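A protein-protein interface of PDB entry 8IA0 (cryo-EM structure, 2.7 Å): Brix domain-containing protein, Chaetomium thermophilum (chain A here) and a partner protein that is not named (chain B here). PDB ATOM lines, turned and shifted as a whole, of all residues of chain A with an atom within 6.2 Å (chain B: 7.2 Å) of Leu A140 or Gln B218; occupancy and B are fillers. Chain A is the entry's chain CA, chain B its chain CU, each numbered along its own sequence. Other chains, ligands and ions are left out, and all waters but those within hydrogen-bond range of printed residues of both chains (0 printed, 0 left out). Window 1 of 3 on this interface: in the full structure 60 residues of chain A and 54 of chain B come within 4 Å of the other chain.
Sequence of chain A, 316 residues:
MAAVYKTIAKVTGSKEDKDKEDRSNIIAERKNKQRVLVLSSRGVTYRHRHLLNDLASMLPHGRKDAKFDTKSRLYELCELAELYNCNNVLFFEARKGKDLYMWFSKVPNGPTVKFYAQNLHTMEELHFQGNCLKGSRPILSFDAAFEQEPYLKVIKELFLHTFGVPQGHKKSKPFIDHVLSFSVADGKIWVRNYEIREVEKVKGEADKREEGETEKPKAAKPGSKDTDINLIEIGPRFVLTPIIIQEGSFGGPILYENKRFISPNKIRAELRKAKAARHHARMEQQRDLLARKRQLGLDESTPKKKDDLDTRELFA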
ATOM      1  N   ARG A 137      -1.270  13.024 -26.778  1.00  0.00           N
ATOM      2  CA  ARG A 137      -1.203  11.579 -26.622  1.00  0.00           C
ATOM      3  C   ARG A 137      -1.365  11.207 -25.156  1.00  0.00           C
ATOM      4  O   ARG A 137      -0.589  11.680 -24.317  1.00  0.00           O
ATOM      5  CB  ARG A 137       0.115  11.047 -27.165  1.00  0.00           C
ATOM      6  CG  ARG A 137       0.305  11.283 -28.647  1.00  0.00           C
ATOM      7  CD  ARG A 137       1.288  10.294 -29.232  1.00  0.00           C
ATOM      8  NE  ARG A 137       0.933   8.920 -28.899  1.00  0.00           N
ATOM      9  CZ  ARG A 137       1.809   7.950 -28.685  1.00  0.00           C
ATOM     10  NH1 ARG A 137       3.111   8.169 -28.752  1.00  0.00           N
ATOM     11  NH2 ARG A 137       1.368   6.730 -28.399  1.00  0.00           N
ATOM     12  N   PRO A 138      -2.339  10.380 -24.803  1.00  0.00           N
ATOM     13  CA  PRO A 138      -2.577  10.051 -23.399  1.00  0.00           C
ATOM     14  C   PRO A 138      -1.783   8.833 -22.946  1.00  0.00           C
ATOM     15  O   PRO A 138      -1.272   8.050 -23.748  1.00  0.00           O
ATOM     16  CB  PRO A 138      -4.079   9.753 -23.378  1.00  0.00           C
ATOM     17  CG  PRO A 138      -4.342   9.167 -24.723  1.00  0.00           C
ATOM     18  CD  PRO A 138      -3.343   9.765 -25.687  1.00  0.00           C
ATOM     19  N   ILE A 139      -1.688   8.691 -21.630  1.00  0.00           N
ATOM     20  CA  ILE A 139      -1.210   7.464 -21.009  1.00  0.00           C
ATOM     21  C   ILE A 139      -2.429   6.604 -20.711  1.00  0.00           C
ATOM     22  O   ILE A 139      -3.363   7.050 -20.037  1.00  0.00           O
ATOM     23  CB  ILE A 139      -0.406   7.751 -19.732  1.00  0.00           C
ATOM     24  CG1 ILE A 139       1.041   8.085 -20.074  1.00  0.00           C
ATOM     25  CG2 ILE A 139      -0.447   6.560 -18.791  1.00  0.00           C
ATOM     26  CD1 ILE A 139       1.842   8.585 -18.898  1.00  0.00           C
ATOM     27  N   LEU A 140      -2.436   5.385 -21.235  1.00  0.00           N
ATOM     28  CA  LEU A 140      -3.545   4.469 -21.023  1.00  0.00           C
ATOM     29  C   LEU A 140      -3.261   3.620 -19.792  1.00  0.00           C
ATOM     30  O   LEU A 140      -2.330   2.808 -19.791  1.00  0.00           O
ATOM     31  CB  LEU A 140      -3.764   3.594 -22.256  1.00  0.00           C
ATOM     32  CG  LEU A 140      -4.184   4.345 -23.520  1.00  0.00           C
ATOM     33  CD1 LEU A 140      -4.626   3.375 -24.599  1.00  0.00           C
ATOM     34  CD2 LEU A 140      -5.287   5.342 -23.212  1.00  0.00           C
ATOM     35  N   SER A 141      -4.057   3.815 -18.746  1.00  0.00           N
ATOM     36  CA  SER A 141      -3.917   3.075 -17.500  1.00  0.00           C
ATOM     37  C   SER A 141      -4.921   1.932 -17.488  1.00  0.00           C
ATOM     38  O   SER A 141      -6.132   2.165 -17.402  1.00  0.00           O
ATOM     39  CB  SER A 141      -4.133   3.988 -16.296  1.00  0.00           C
ATOM     40  OG  SER A 141      -4.310   3.229 -15.113  1.00  0.00           O
ATOM     41  N   PHE A 142      -4.422   0.707 -17.572  1.00  0.00           N
ATOM     42  CA  PHE A 142      -5.254  -0.484 -17.548  1.00  0.00           C
ATOM     43  C   PHE A 142      -5.095  -1.177 -16.197  1.00  0.00           C
ATOM     44  O   PHE A 142      -4.135  -0.940 -15.459  1.00  0.00           O
ATOM     45  CB  PHE A 142      -4.897  -1.409 -18.712  1.00  0.00           C
ATOM     46  CG  PHE A 142      -5.459  -0.964 -20.029  1.00  0.00           C
ATOM     47  CD1 PHE A 142      -6.801  -1.125 -20.312  1.00  0.00           C
ATOM     48  CD2 PHE A 142      -4.645  -0.377 -20.981  1.00  0.00           C
ATOM     49  CE1 PHE A 142      -7.321  -0.714 -21.520  1.00  0.00           C
ATOM     50  CE2 PHE A 142      -5.161   0.037 -22.191  1.00  0.00           C
ATOM     51  CZ  PHE A 142      -6.500  -0.131 -22.460  1.00  0.00           C
ATOM     52  N   PHE A 159      -9.683  -1.093 -26.923  1.00  0.00           N
ATOM     53  CA  PHE A 159      -9.491   0.218 -26.314  1.00  0.00           C
ATOM     54  C   PHE A 159      -8.161   0.832 -26.731  1.00  0.00           C
ATOM     55  O   PHE A 159      -8.076   2.043 -26.960  1.00  0.00           O
ATOM     56  CB  PHE A 159      -9.574   0.105 -24.794  1.00  0.00           C
ATOM     57  CG  PHE A 159     -10.974   0.007 -24.271  1.00  0.00           C
ATOM     58  CD1 PHE A 159     -12.056   0.221 -25.106  1.00  0.00           C
ATOM     59  CD2 PHE A 159     -11.210  -0.301 -22.946  1.00  0.00           C
ATOM     60  CE1 PHE A 159     -13.344   0.131 -24.627  1.00  0.00           C
ATOM     61  CE2 PHE A 159     -12.497  -0.391 -22.461  1.00  0.00           C
ATOM     62  CZ  PHE A 159     -13.564  -0.177 -23.303  1.00  0.00           C
ATOM     63  N   LEU A 160      -7.113   0.014 -26.831  1.00  0.00           N
ATOM     64  CA  LEU A 160      -5.805   0.531 -27.221  1.00  0.00           C
ATOM     65  C   LEU A 160      -5.822   1.034 -28.660  1.00  0.00           C
ATOM     66  O   LEU A 160      -5.050   1.928 -29.021  1.00  0.00           O
ATOM     67  CB  LEU A 160      -4.743  -0.552 -27.025  1.00  0.00           C
ATOM     68  CG  LEU A 160      -3.286  -0.149 -26.786  1.00  0.00           C
ATOM     69  CD1 LEU A 160      -2.536  -1.302 -26.145  1.00  0.00           C
ATOM     70  CD2 LEU A 160      -2.588   0.267 -28.068  1.00  0.00           C
ATOM     71  N   HIS A 161      -6.704   0.481 -29.493  1.00  0.00           N
ATOM     72  CA  HIS A 161      -6.807   0.950 -30.871  1.00  0.00           C
ATOM     73  C   HIS A 161      -7.688   2.190 -30.972  1.00  0.00           C
ATOM     74  O   HIS A 161      -7.418   3.085 -31.780  1.00  0.00           O
ATOM     75  CB  HIS A 161      -7.350  -0.162 -31.767  1.00  0.00           C
ATOM     76  CG  HIS A 161      -6.440  -1.343 -31.887  1.00  0.00           C
ATOM     77  ND1 HIS A 161      -6.579  -2.291 -32.876  1.00  0.00           N
ATOM     78  CD2 HIS A 161      -5.374  -1.729 -31.145  1.00  0.00           C
ATOM     79  CE1 HIS A 161      -5.643  -3.211 -32.738  1.00  0.00           C
ATOM     80  NE2 HIS A 161      -4.900  -2.895 -31.693  1.00  0.00           N
ATOM     81  N   PHE A 163      -8.350   4.500 -28.515  1.00  0.00           N
ATOM     82  CA  PHE A 163      -7.727   5.626 -27.830  1.00  0.00           C
ATOM     83  C   PHE A 163      -6.213   5.642 -28.021  1.00  0.00           C
ATOM     84  O   PHE A 163      -5.483   6.185 -27.189  1.00  0.00           O
ATOM     85  CB  PHE A 163      -8.067   5.606 -26.342  1.00  0.00           C
ATOM     86  CG  PHE A 163      -9.527   5.415 -26.054  1.00  0.00           C
ATOM     87  CD1 PHE A 163     -10.413   6.468 -26.164  1.00  0.00           C
ATOM     88  CD2 PHE A 163     -10.009   4.182 -25.660  1.00  0.00           C
ATOM     89  CE1 PHE A 163     -11.752   6.292 -25.897  1.00  0.00           C
ATOM     90  CE2 PHE A 163     -11.348   4.001 -25.392  1.00  0.00           C
ATOM     91  CZ  PHE A 163     -12.220   5.057 -25.510  1.00  0.00           C
ATOM     92  N   GLY A 164      -5.729   5.047 -29.111  1.00  0.00           N
ATOM     93  CA  GLY A 164      -4.292   4.939 -29.302  1.00  0.00           C
ATOM     94  C   GLY A 164      -3.616   6.280 -29.510  1.00  0.00           C
ATOM     95  O   GLY A 164      -2.582   6.566 -28.901  1.00  0.00           O
ATOM     96  N   GLN A 167       1.584   7.495 -32.896  1.00  0.00           N
ATOM     97  CA  GLN A 167       2.730   8.248 -32.395  1.00  0.00           C
ATOM     98  C   GLN A 167       3.030   9.469 -33.255  1.00  0.00           C
ATOM     99  O   GLN A 167       3.194  10.580 -32.740  1.00  0.00           O
ATOM    100  CB  GLN A 167       3.951   7.333 -32.316  1.00  0.00           C
ATOM    101  CG  GLN A 167       5.075   7.870 -31.462  1.00  0.00           C
ATOM    102  CD  GLN A 167       6.424   7.334 -31.880  1.00  0.00           C
ATOM    103  OE1 GLN A 167       6.512   6.375 -32.646  1.00  0.00           O
ATOM    104  NE2 GLN A 167       7.487   7.948 -31.377  1.00  0.00           N
ATOM    105  N   ILE A 176       2.663  15.679 -23.307  1.00  0.00           N
ATOM    106  CA  ILE A 176       1.724  14.745 -22.699  1.00  0.00           C
ATOM    107  C   ILE A 176       1.367  15.230 -21.300  1.00  0.00           C
ATOM    108  O   ILE A 176       2.253  15.462 -20.468  1.00  0.00           O
ATOM    109  CB  ILE A 176       2.310  13.324 -22.665  1.00  0.00           C
ATOM    110  CG1 ILE A 176       1.536  12.440 -21.693  1.00  0.00           C
ATOM    111  CG2 ILE A 176       3.787  13.362 -22.329  1.00  0.00           C
ATOM    112  CD1 ILE A 176       1.998  11.016 -21.709  1.00  0.00           C
ATOM    113  N   VAL A 179      -3.943  11.426 -18.425  1.00  0.00           N
ATOM    114  CA  VAL A 179      -3.966   9.970 -18.369  1.00  0.00           C
ATOM    115  C   VAL A 179      -5.415   9.505 -18.396  1.00  0.00           C
ATOM    116  O   VAL A 179      -6.255  10.023 -17.651  1.00  0.00           O
ATOM    117  CB  VAL A 179      -3.235   9.439 -17.120  1.00  0.00           C
ATOM    118  CG1 VAL A 179      -3.719  10.148 -15.865  1.00  0.00           C
ATOM    119  CG2 VAL A 179      -3.428   7.941 -16.980  1.00  0.00           C
ATOM    120  N   LEU A 180      -5.708   8.542 -19.264  1.00  0.00           N
ATOM    121  CA  LEU A 180      -7.019   7.910 -19.339  1.00  0.00           C
ATOM    122  C   LEU A 180      -6.930   6.543 -18.671  1.00  0.00           C
ATOM    123  O   LEU A 180      -6.113   5.707 -19.069  1.00  0.00           O
ATOM    124  CB  LEU A 180      -7.478   7.786 -20.792  1.00  0.00           C
ATOM    125  CG  LEU A 180      -8.894   7.286 -21.082  1.00  0.00           C
ATOM    126  CD1 LEU A 180      -9.946   8.200 -20.486  1.00  0.00           C
ATOM    127  CD2 LEU A 180      -9.099   7.152 -22.579  1.00  0.00           C
ATOM    128  N   SER A 181      -7.769   6.318 -17.665  1.00  0.00           N
ATOM    129  CA  SER A 181      -7.667   5.151 -16.800  1.00  0.00           C
ATOM    130  C   SER A 181      -8.890   4.260 -16.956  1.00  0.00           C
ATOM    131  O   SER A 181     -10.026   4.746 -16.935  1.00  0.00           O
ATOM    132  CB  SER A 181      -7.513   5.574 -15.338  1.00  0.00           C
ATOM    133  OG  SER A 181      -7.598   4.458 -14.472  1.00  0.00           O
ATOM    134  N   PHE A 182      -8.653   2.960 -17.107  1.00  0.00           N
ATOM    135  CA  PHE A 182      -9.705   1.956 -17.175  1.00  0.00           C
ATOM    136  C   PHE A 182      -9.569   1.015 -15.988  1.00  0.00           C
ATOM    137  O   PHE A 182      -8.501   0.437 -15.770  1.00  0.00           O
ATOM    138  CB  PHE A 182      -9.640   1.165 -18.483  1.00  0.00           C
ATOM    139  CG  PHE A 182      -9.609   2.022 -19.712  1.00  0.00           C
ATOM    140  CD1 PHE A 182     -10.782   2.403 -20.334  1.00  0.00           C
ATOM    141  CD2 PHE A 182      -8.407   2.440 -20.250  1.00  0.00           C
ATOM    142  CE1 PHE A 182     -10.757   3.188 -21.465  1.00  0.00           C
ATOM    143  CE2 PHE A 182      -8.376   3.225 -21.383  1.00  0.00           C
ATOM    144  CZ  PHE A 182      -9.553   3.598 -21.991  1.00  0.00           C
ATOM    145  N   ILE B 207       3.266  -5.185 -28.747  1.00  0.00           N
ATOM    146  CA  ILE B 207       3.432  -4.292 -27.609  1.00  0.00           C
ATOM    147  C   ILE B 207       4.566  -4.729 -26.693  1.00  0.00           C
ATOM    148  O   ILE B 207       4.693  -4.201 -25.585  1.00  0.00           O
ATOM    149  CB  ILE B 207       2.116  -4.165 -26.812  1.00  0.00           C
ATOM    150  CG1 ILE B 207       0.912  -4.226 -27.753  1.00  0.00           C
ATOM    151  CG2 ILE B 207       2.052  -2.854 -26.069  1.00  0.00           C
ATOM    152  CD1 ILE B 207       0.786  -3.024 -28.669  1.00  0.00           C
ATOM    153  N   PRO B 213       9.237   0.287 -28.179  1.00  0.00           N
ATOM    154  CA  PRO B 213       9.410   1.310 -27.142  1.00  0.00           C
ATOM    155  C   PRO B 213       8.078   1.790 -26.588  1.00  0.00           C
ATOM    156  O   PRO B 213       7.024   1.634 -27.207  1.00  0.00           O
ATOM    157  CB  PRO B 213      10.150   2.438 -27.870  1.00  0.00           C
ATOM    158  CG  PRO B 213       9.918   2.186 -29.317  1.00  0.00           C
ATOM    159  CD  PRO B 213       9.802   0.707 -29.470  1.00  0.00           C
ATOM    160  N   PHE B 214       8.142   2.377 -25.390  1.00  0.00           N
ATOM    161  CA  PHE B 214       6.930   2.794 -24.692  1.00  0.00           C
ATOM    162  C   PHE B 214       6.199   3.906 -25.429  1.00  0.00           C
ATOM    163  O   PHE B 214       4.984   4.063 -25.265  1.00  0.00           O
ATOM    164  CB  PHE B 214       7.279   3.236 -23.272  1.00  0.00           C
ATOM    165  CG  PHE B 214       6.100   3.702 -22.470  1.00  0.00           C
ATOM    166  CD1 PHE B 214       5.201   2.796 -21.940  1.00  0.00           C
ATOM    167  CD2 PHE B 214       5.900   5.050 -22.237  1.00  0.00           C
ATOM    168  CE1 PHE B 214       4.119   3.228 -21.198  1.00  0.00           C
ATOM    169  CE2 PHE B 214       4.822   5.483 -21.497  1.00  0.00           C
ATOM    170  CZ  PHE B 214       3.932   4.572 -20.976  1.00  0.00           C
ATOM    171  N   SER B 215       6.912   4.689 -26.239  1.00  0.00           N
ATOM    172  CA  SER B 215       6.274   5.788 -26.954  1.00  0.00           C
ATOM    173  C   SER B 215       5.268   5.276 -27.978  1.00  0.00           C
ATOM    174  O   SER B 215       4.342   5.998 -28.366  1.00  0.00           O
ATOM    175  CB  SER B 215       7.334   6.655 -27.631  1.00  0.00           C
ATOM    176  OG  SER B 215       6.738   7.701 -28.378  1.00  0.00           O
ATOM    177  N   PHE B 216       5.433   4.032 -28.425  1.00  0.00           N
ATOM    178  CA  PHE B 216       4.568   3.491 -29.469  1.00  0.00           C
ATOM    179  C   PHE B 216       3.154   3.255 -28.954  1.00  0.00           C
ATOM    180  O   PHE B 216       2.175   3.625 -29.612  1.00  0.00           O
ATOM    181  CB  PHE B 216       5.175   2.199 -30.017  1.00  0.00           C
ATOM    182  CG  PHE B 216       4.360   1.553 -31.097  1.00  0.00           C
ATOM    183  CD1 PHE B 216       4.447   1.995 -32.403  1.00  0.00           C
ATOM    184  CD2 PHE B 216       3.521   0.492 -30.809  1.00  0.00           C
ATOM    185  CE1 PHE B 216       3.703   1.401 -33.395  1.00  0.00           C
ATOM    186  CE2 PHE B 216       2.777  -0.105 -31.800  1.00  0.00           C
ATOM    187  CZ  PHE B 216       2.867   0.350 -33.095  1.00  0.00           C
ATOM    188  N   HIS B 217       3.025   2.642 -27.780  1.00  0.00           N
ATOM    189  CA  HIS B 217       1.724   2.264 -27.240  1.00  0.00           C
ATOM    190  C   HIS B 217       1.270   3.145 -26.084  1.00  0.00           C
ATOM    191  O   HIS B 217       0.090   3.500 -26.017  1.00  0.00           O
ATOM    192  CB  HIS B 217       1.740   0.800 -26.786  1.00  0.00           C
ATOM    193  CG  HIS B 217       2.851   0.465 -25.839  1.00  0.00           C
ATOM    194  ND1 HIS B 217       2.626  -0.090 -24.598  1.00  0.00           N
ATOM    195  CD2 HIS B 217       4.195   0.574 -25.963  1.00  0.00           C
ATOM    196  CE1 HIS B 217       3.781  -0.292 -23.991  1.00  0.00           C
ATOM    197  NE2 HIS B 217       4.749   0.104 -24.797  1.00  0.00           N
ATOM    198  N   GLN B 218       2.178   3.500 -25.173  1.00  0.00           N
ATOM    199  CA  GLN B 218       1.861   4.344 -24.017  1.00  0.00           C
ATOM    200  C   GLN B 218       0.750   3.735 -23.166  1.00  0.00           C
ATOM    201  O   GLN B 218      -0.121   4.439 -22.653  1.00  0.00           O
ATOM    202  CB  GLN B 218       1.492   5.763 -24.452  1.00  0.00           C
ATOM    203  CG  GLN B 218       2.595   6.486 -25.195  1.00  0.00           C
ATOM    204  CD  GLN B 218       2.566   7.978 -24.967  1.00  0.00           C
ATOM    205  OE1 GLN B 218       1.717   8.489 -24.241  1.00  0.00           O
ATOM    206  NE2 GLN B 218       3.495   8.689 -25.591  1.00  0.00           N
ATOM    207  N   SER B 219       0.784   2.416 -23.009  1.00  0.00           N
ATOM    208  CA  SER B 219      -0.173   1.696 -22.184  1.00  0.00           C
ATOM    209  C   SER B 219       0.555   1.017 -21.035  1.00  0.00           C
ATOM    210  O   SER B 219       1.622   0.427 -21.227  1.00  0.00           O
ATOM    211  CB  SER B 219      -0.945   0.657 -23.002  1.00  0.00           C
ATOM    212  OG  SER B 219      -0.080  -0.358 -23.481  1.00  0.00           O
ATOM    213  N   VAL B 220      -0.023   1.105 -19.841  1.00  0.00           N
ATOM    214  CA  VAL B 220       0.532   0.489 -18.643  1.00  0.00           C
ATOM    215  C   VAL B 220      -0.545  -0.377 -18.010  1.00  0.00           C
ATOM    216  O   VAL B 220      -1.680   0.074 -17.824  1.00  0.00           O
ATOM    217  CB  VAL B 220       1.037   1.541 -17.636  1.00  0.00           C
ATOM    218  CG1 VAL B 220       1.546   0.867 -16.374  1.00  0.00           C
ATOM    219  CG2 VAL B 220       2.122   2.399 -18.263  1.00  0.00           C
ATOM    220  N   VAL B 221      -0.194  -1.618 -17.684  1.00  0.00           N
ATOM    221  CA  VAL B 221      -1.094  -2.546 -17.014  1.00  0.00           C
ATOM    222  C   VAL B 221      -0.693  -2.623 -15.548  1.00  0.00           C
ATOM    223  O   VAL B 221       0.462  -2.931 -15.229  1.00  0.00           O
ATOM    224  CB  VAL B 221      -1.063  -3.938 -17.668  1.00  0.00           C
ATOM    225  CG1 VAL B 221      -2.019  -4.876 -16.956  1.00  0.00           C
ATOM    226  CG2 VAL B 221      -1.412  -3.835 -19.142  1.00  0.00           C
ATOM    227  N   GLN B 246      -4.621   3.967  -9.082  1.00  0.00           N
ATOM    228  CA  GLN B 246      -4.228   3.166 -10.238  1.00  0.00           C
ATOM    229  C   GLN B 246      -3.696   4.047 -11.361  1.00  0.00           C
ATOM    230  O   GLN B 246      -2.670   3.736 -11.977  1.00  0.00           O
ATOM    231  CB  GLN B 246      -5.416   2.338 -10.726  1.00  0.00           C
ATOM    232  CG  GLN B 246      -5.107   1.472 -11.932  1.00  0.00           C
ATOM    233  CD  GLN B 246      -6.332   1.192 -12.775  1.00  0.00           C
ATOM    234  OE1 GLN B 246      -7.454   1.176 -12.273  1.00  0.00           O
ATOM    235  NE2 GLN B 246      -6.123   0.967 -14.065  1.00  0.00           N
ATOM    236  N   ALA B 250       0.399   4.560 -13.169  1.00  0.00           N
ATOM    237  CA  ALA B 250       0.659   4.509 -14.604  1.00  0.00           C
ATOM    238  C   ALA B 250       1.268   5.813 -15.100  1.00  0.00           C
ATOM    239  O   ALA B 250       2.178   5.801 -15.936  1.00  0.00           O
ATOM    240  CB  ALA B 250      -0.629   4.194 -15.362  1.00  0.00           C
ATOM    241  N   GLY B 254       4.856   5.891 -16.514  1.00  0.00           N
ATOM    242  CA  GLY B 254       4.911   6.406 -17.871  1.00  0.00           C
ATOM    243  C   GLY B 254       5.898   7.545 -18.027  1.00  0.00           C
ATOM    244  O   GLY B 254       6.619   7.621 -19.025  1.00  0.00           O
ATOM    245  N   LEU B 258       9.131   7.478 -20.481  1.00  0.00           N
ATOM    246  CA  LEU B 258       9.160   8.465 -21.555  1.00  0.00           C
ATOM    247  C   LEU B 258      10.400   9.347 -21.467  1.00  0.00           C
ATOM    248  O   LEU B 258      11.031   9.643 -22.487  1.00  0.00           O
ATOM    249  CB  LEU B 258       7.894   9.319 -21.517  1.00  0.00           C
ATOM    250  CG  LEU B 258       6.652   8.718 -22.174  1.00  0.00           C
ATOM    251  CD1 LEU B 258       5.431   9.574 -21.889  1.00  0.00           C
ATOM    252  CD2 LEU B 258       6.860   8.556 -23.669  1.00  0.00           C
ATOM    253  N   GLU B 261      13.347   7.538 -22.731  1.00  0.00           N
ATOM    254  CA  GLU B 261      13.339   7.477 -24.186  1.00  0.00           C
ATOM    255  C   GLU B 261      13.599   8.833 -24.830  1.00  0.00           C
ATOM    256  O   GLU B 261      14.066   8.881 -25.972  1.00  0.00           O
ATOM    257  CB  GLU B 261      12.004   6.911 -24.674  1.00  0.00           C
ATOM    258  CG  GLU B 261      11.951   6.614 -26.157  1.00  0.00           C
ATOM    259  CD  GLU B 261      10.665   5.929 -26.564  1.00  0.00           C
ATOM    260  OE1 GLU B 261       9.822   5.672 -25.680  1.00  0.00           O
ATOM    261  OE2 GLU B 261      10.496   5.649 -27.769  1.00  0.00           O
ATOM    262  N   VAL B 263      11.170  11.442 -25.028  1.00  0.00           N
ATOM    263  CA  VAL B 263       9.959  12.122 -25.491  1.00  0.00           C
ATOM    264  C   VAL B 263       9.636  13.261 -24.527  1.00  0.00           C
ATOM    265  O   VAL B 263       9.589  13.031 -23.309  1.00  0.00           O
ATOM    266  CB  VAL B 263       8.797  11.141 -25.589  1.00  0.00           C
ATOM    267  CG1 VAL B 263       7.502  11.879 -25.884  1.00  0.00           C
ATOM    268  CG2 VAL B 263       9.077  10.099 -26.658  1.00  0.00           C
ATOM    269  N   PRO B 264       9.429  14.482 -25.019  1.00  0.00           N
ATOM    270  CA  PRO B 264       9.103  15.594 -24.119  1.00  0.00           C
ATOM    271  C   PRO B 264       7.814  15.333 -23.355  1.00  0.00           C
ATOM    272  O   PRO B 264       6.854  14.779 -23.892  1.00  0.00           O
ATOM    273  CB  PRO B 264       8.964  16.787 -25.070  1.00  0.00           C
ATOM    274  CG  PRO B 264       9.737  16.397 -26.282  1.00  0.00           C
ATOM    275  CD  PRO B 264       9.545  14.923 -26.417  1.00  0.00           C
ATOM    276  N   PHE B 265       7.803  15.742 -22.088  1.00  0.00           N
ATOM    277  CA  PHE B 265       6.681  15.471 -21.196  1.00  0.00           C
ATOM    278  C   PHE B 265       6.015  16.748 -20.703  1.00  0.00           C
ATOM    279  O   PHE B 265       4.797  16.894 -20.846  1.00  0.00           O
ATOM    280  CB  PHE B 265       7.164  14.617 -20.015  1.00  0.00           C
ATOM    281  CG  PHE B 265       6.055  13.974 -19.236  1.00  0.00           C
ATOM    282  CD1 PHE B 265       5.420  14.659 -18.216  1.00  0.00           C
ATOM    283  CD2 PHE B 265       5.655  12.681 -19.514  1.00  0.00           C
ATOM    284  CE1 PHE B 265       4.403  14.071 -17.498  1.00  0.00           C
ATOM    285  CE2 PHE B 265       4.638  12.090 -18.800  1.00  0.00           C
ATOM    286  CZ  PHE B 265       4.013  12.785 -17.790  1.00  0.00           C
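The backbone NH (N) of Val B263 is in hydrogen-bond range of the backbone carbonyl oxygen (O) of Leu B258, at 3.1 Å.
The backbone NH (N) of Leu A180 sits at hydrogen-bond distance from the backbone carbonyl oxygen (O) of Ile A139, 2.9 Å away.
OG of Ser B219 lies within hydrogen-bond range of ND1 of His B217 (2.9 Å).
The backbone carbonyl oxygen (O) of Ser A141 sits at hydrogen-bond distance from the backbone NH (N) of Phe A182, at 2.7 Å.
N of Ser A141 lies within hydrogen-bond range of O of Leu A180 (2.8 Å).
The backbone NH (N) of Ser B215 sits at hydrogen-bond distance from the side-chain carboxylate (OE1) of Glu B261 (3.1 Å).
N of Phe A142 sits at hydrogen-bond distance from O of Val B220, 2.8 Å away.
The side-chain amide nitrogen of Gln B246 sits at hydrogen-bond distance from the backbone carbonyl oxygen of Phe A142 (3.1 Å).
The guanidinium group of Arg A137 lies within hydrogen-bond range of the backbone carbonyl oxygen of Ser B215, 2.5 Å away.
N of Leu A140 is in hydrogen-bond range of O of Gln B218 (2.9 Å).
The side-chain hydroxyl (OG) of Ser A141 is in hydrogen-bond range of the side-chain amide nitrogen (NE2) of Gln B246.
The backbone carbonyl oxygen (O) of Phe B265 is in hydrogen-bond range of the backbone NH (N) of Ile A176 (3.5 Å).
O of Leu A140 is in hydrogen-bond range of N of Val B220 (2.9 Å).
NE2 of Gln B218 sits close to NH1 of Arg A137 (3.2 Å).
The side-chain hydroxyl (OG) of Ser B215 is in hydrogen-bond range of the side-chain amide nitrogen (NE2) of Gln A167 (3.1 Å).
The backbone carbonyl oxygen of Pro A138 sits close to the side-chain amide oxygen of Gln B218 (3.1 Å).
O of Phe A182 sits at hydrogen-bond distance from NE2 of Gln B246.
The backbone carbonyl oxygen (O) of Phe B216 sits at hydrogen-bond distance from the guanidinium group (NH2) of Arg A137 (3.4 Å).
Gln B218 touches Ile A139 (O to CA, 3.6 Å).
O of Ala B250 touches CG2 of Ile A139, 3.95 Å away.
Ser A141 touches Val B220.
Ala B250 touches Ser A141.
CA of Val B221 touches O of Phe A142, at 3.8 Å.
Ser B219 touches Leu A160 (OG to CD1, 3.7 Å).
CD1 of Ile A176 touches OE1 of Gln B218, 3.6 Å away.
Leu B258 touches Ile A176 (CD1 to CD1, 3.7 Å).
Ile A176 touches Pro B264 (CG2 to O, 3.7 Å).
Gln B246 touches Ser A181 (NE2 to OG, 3.8 Å).
Of the 18 printed residues of chain B, 12 touch a printed residue of chain A.
Printed residues of chain B that touch a printed residue of chain A: Ser B215, Phe B216, Gln B218, Ser B219, Val B220, Val B221, Gln B246, Ala B250, Gly B254, Leu B258, Pro B264 and Phe B265.
Of the 17 printed residues of chain A, 11 touch a printed residue of chain B.
Printed residues of chain A that touch a printed residue of chain B: Arg A137, Pro A138, Ile A139, Leu A140, Ser A141, Phe A142, Leu A160, Gln A167, Ile A176, Ser A181 and Phe A182.
Hydrophobic or aromatic side chains of chain A within 4 Å of the printed part of chain B: Ile A139, Leu A140, Phe A142, Leu A160 and Ile A176.
Along chain A the printed residues that touch a printed residue of chain B span positions 137 to 182.
Among the printed residues, no Asp or Glu carboxylate lies within 4 Å of a Lys or Arg side-chain nitrogen of the other chain.
Leu A140 touches just these residues of chain B: Gln B218 (2.9 Å), Ser B219 (3.4 Å) and Val B220 (2.9 Å).
Of chain A, only Arg A137, Pro A138, Ile A139, Leu A140 and Ile A176 come within 4 Å of Gln B218.
Printed residues of chain A within 4 Å of Gln B246: Ser A141 (3.1 Å), Phe A142 (3.1 Å), Ser A181 (3.8 Å) and Phe A182 (3.0 Å).
Printed residues of chain A within 4 Å of Leu B258: Ile A176 (3.7 Å).
Glu B261 touches none of the printed residues of chain A.
Val B263 touches none of the printed residues of chain A.
The nearest residue of chain A that does not touch Gln B218 is Ser A141 (5.6 Å).
The nearest printed residue of chain A that does not touch Ser B219 is Phe A142 (4.3 Å).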
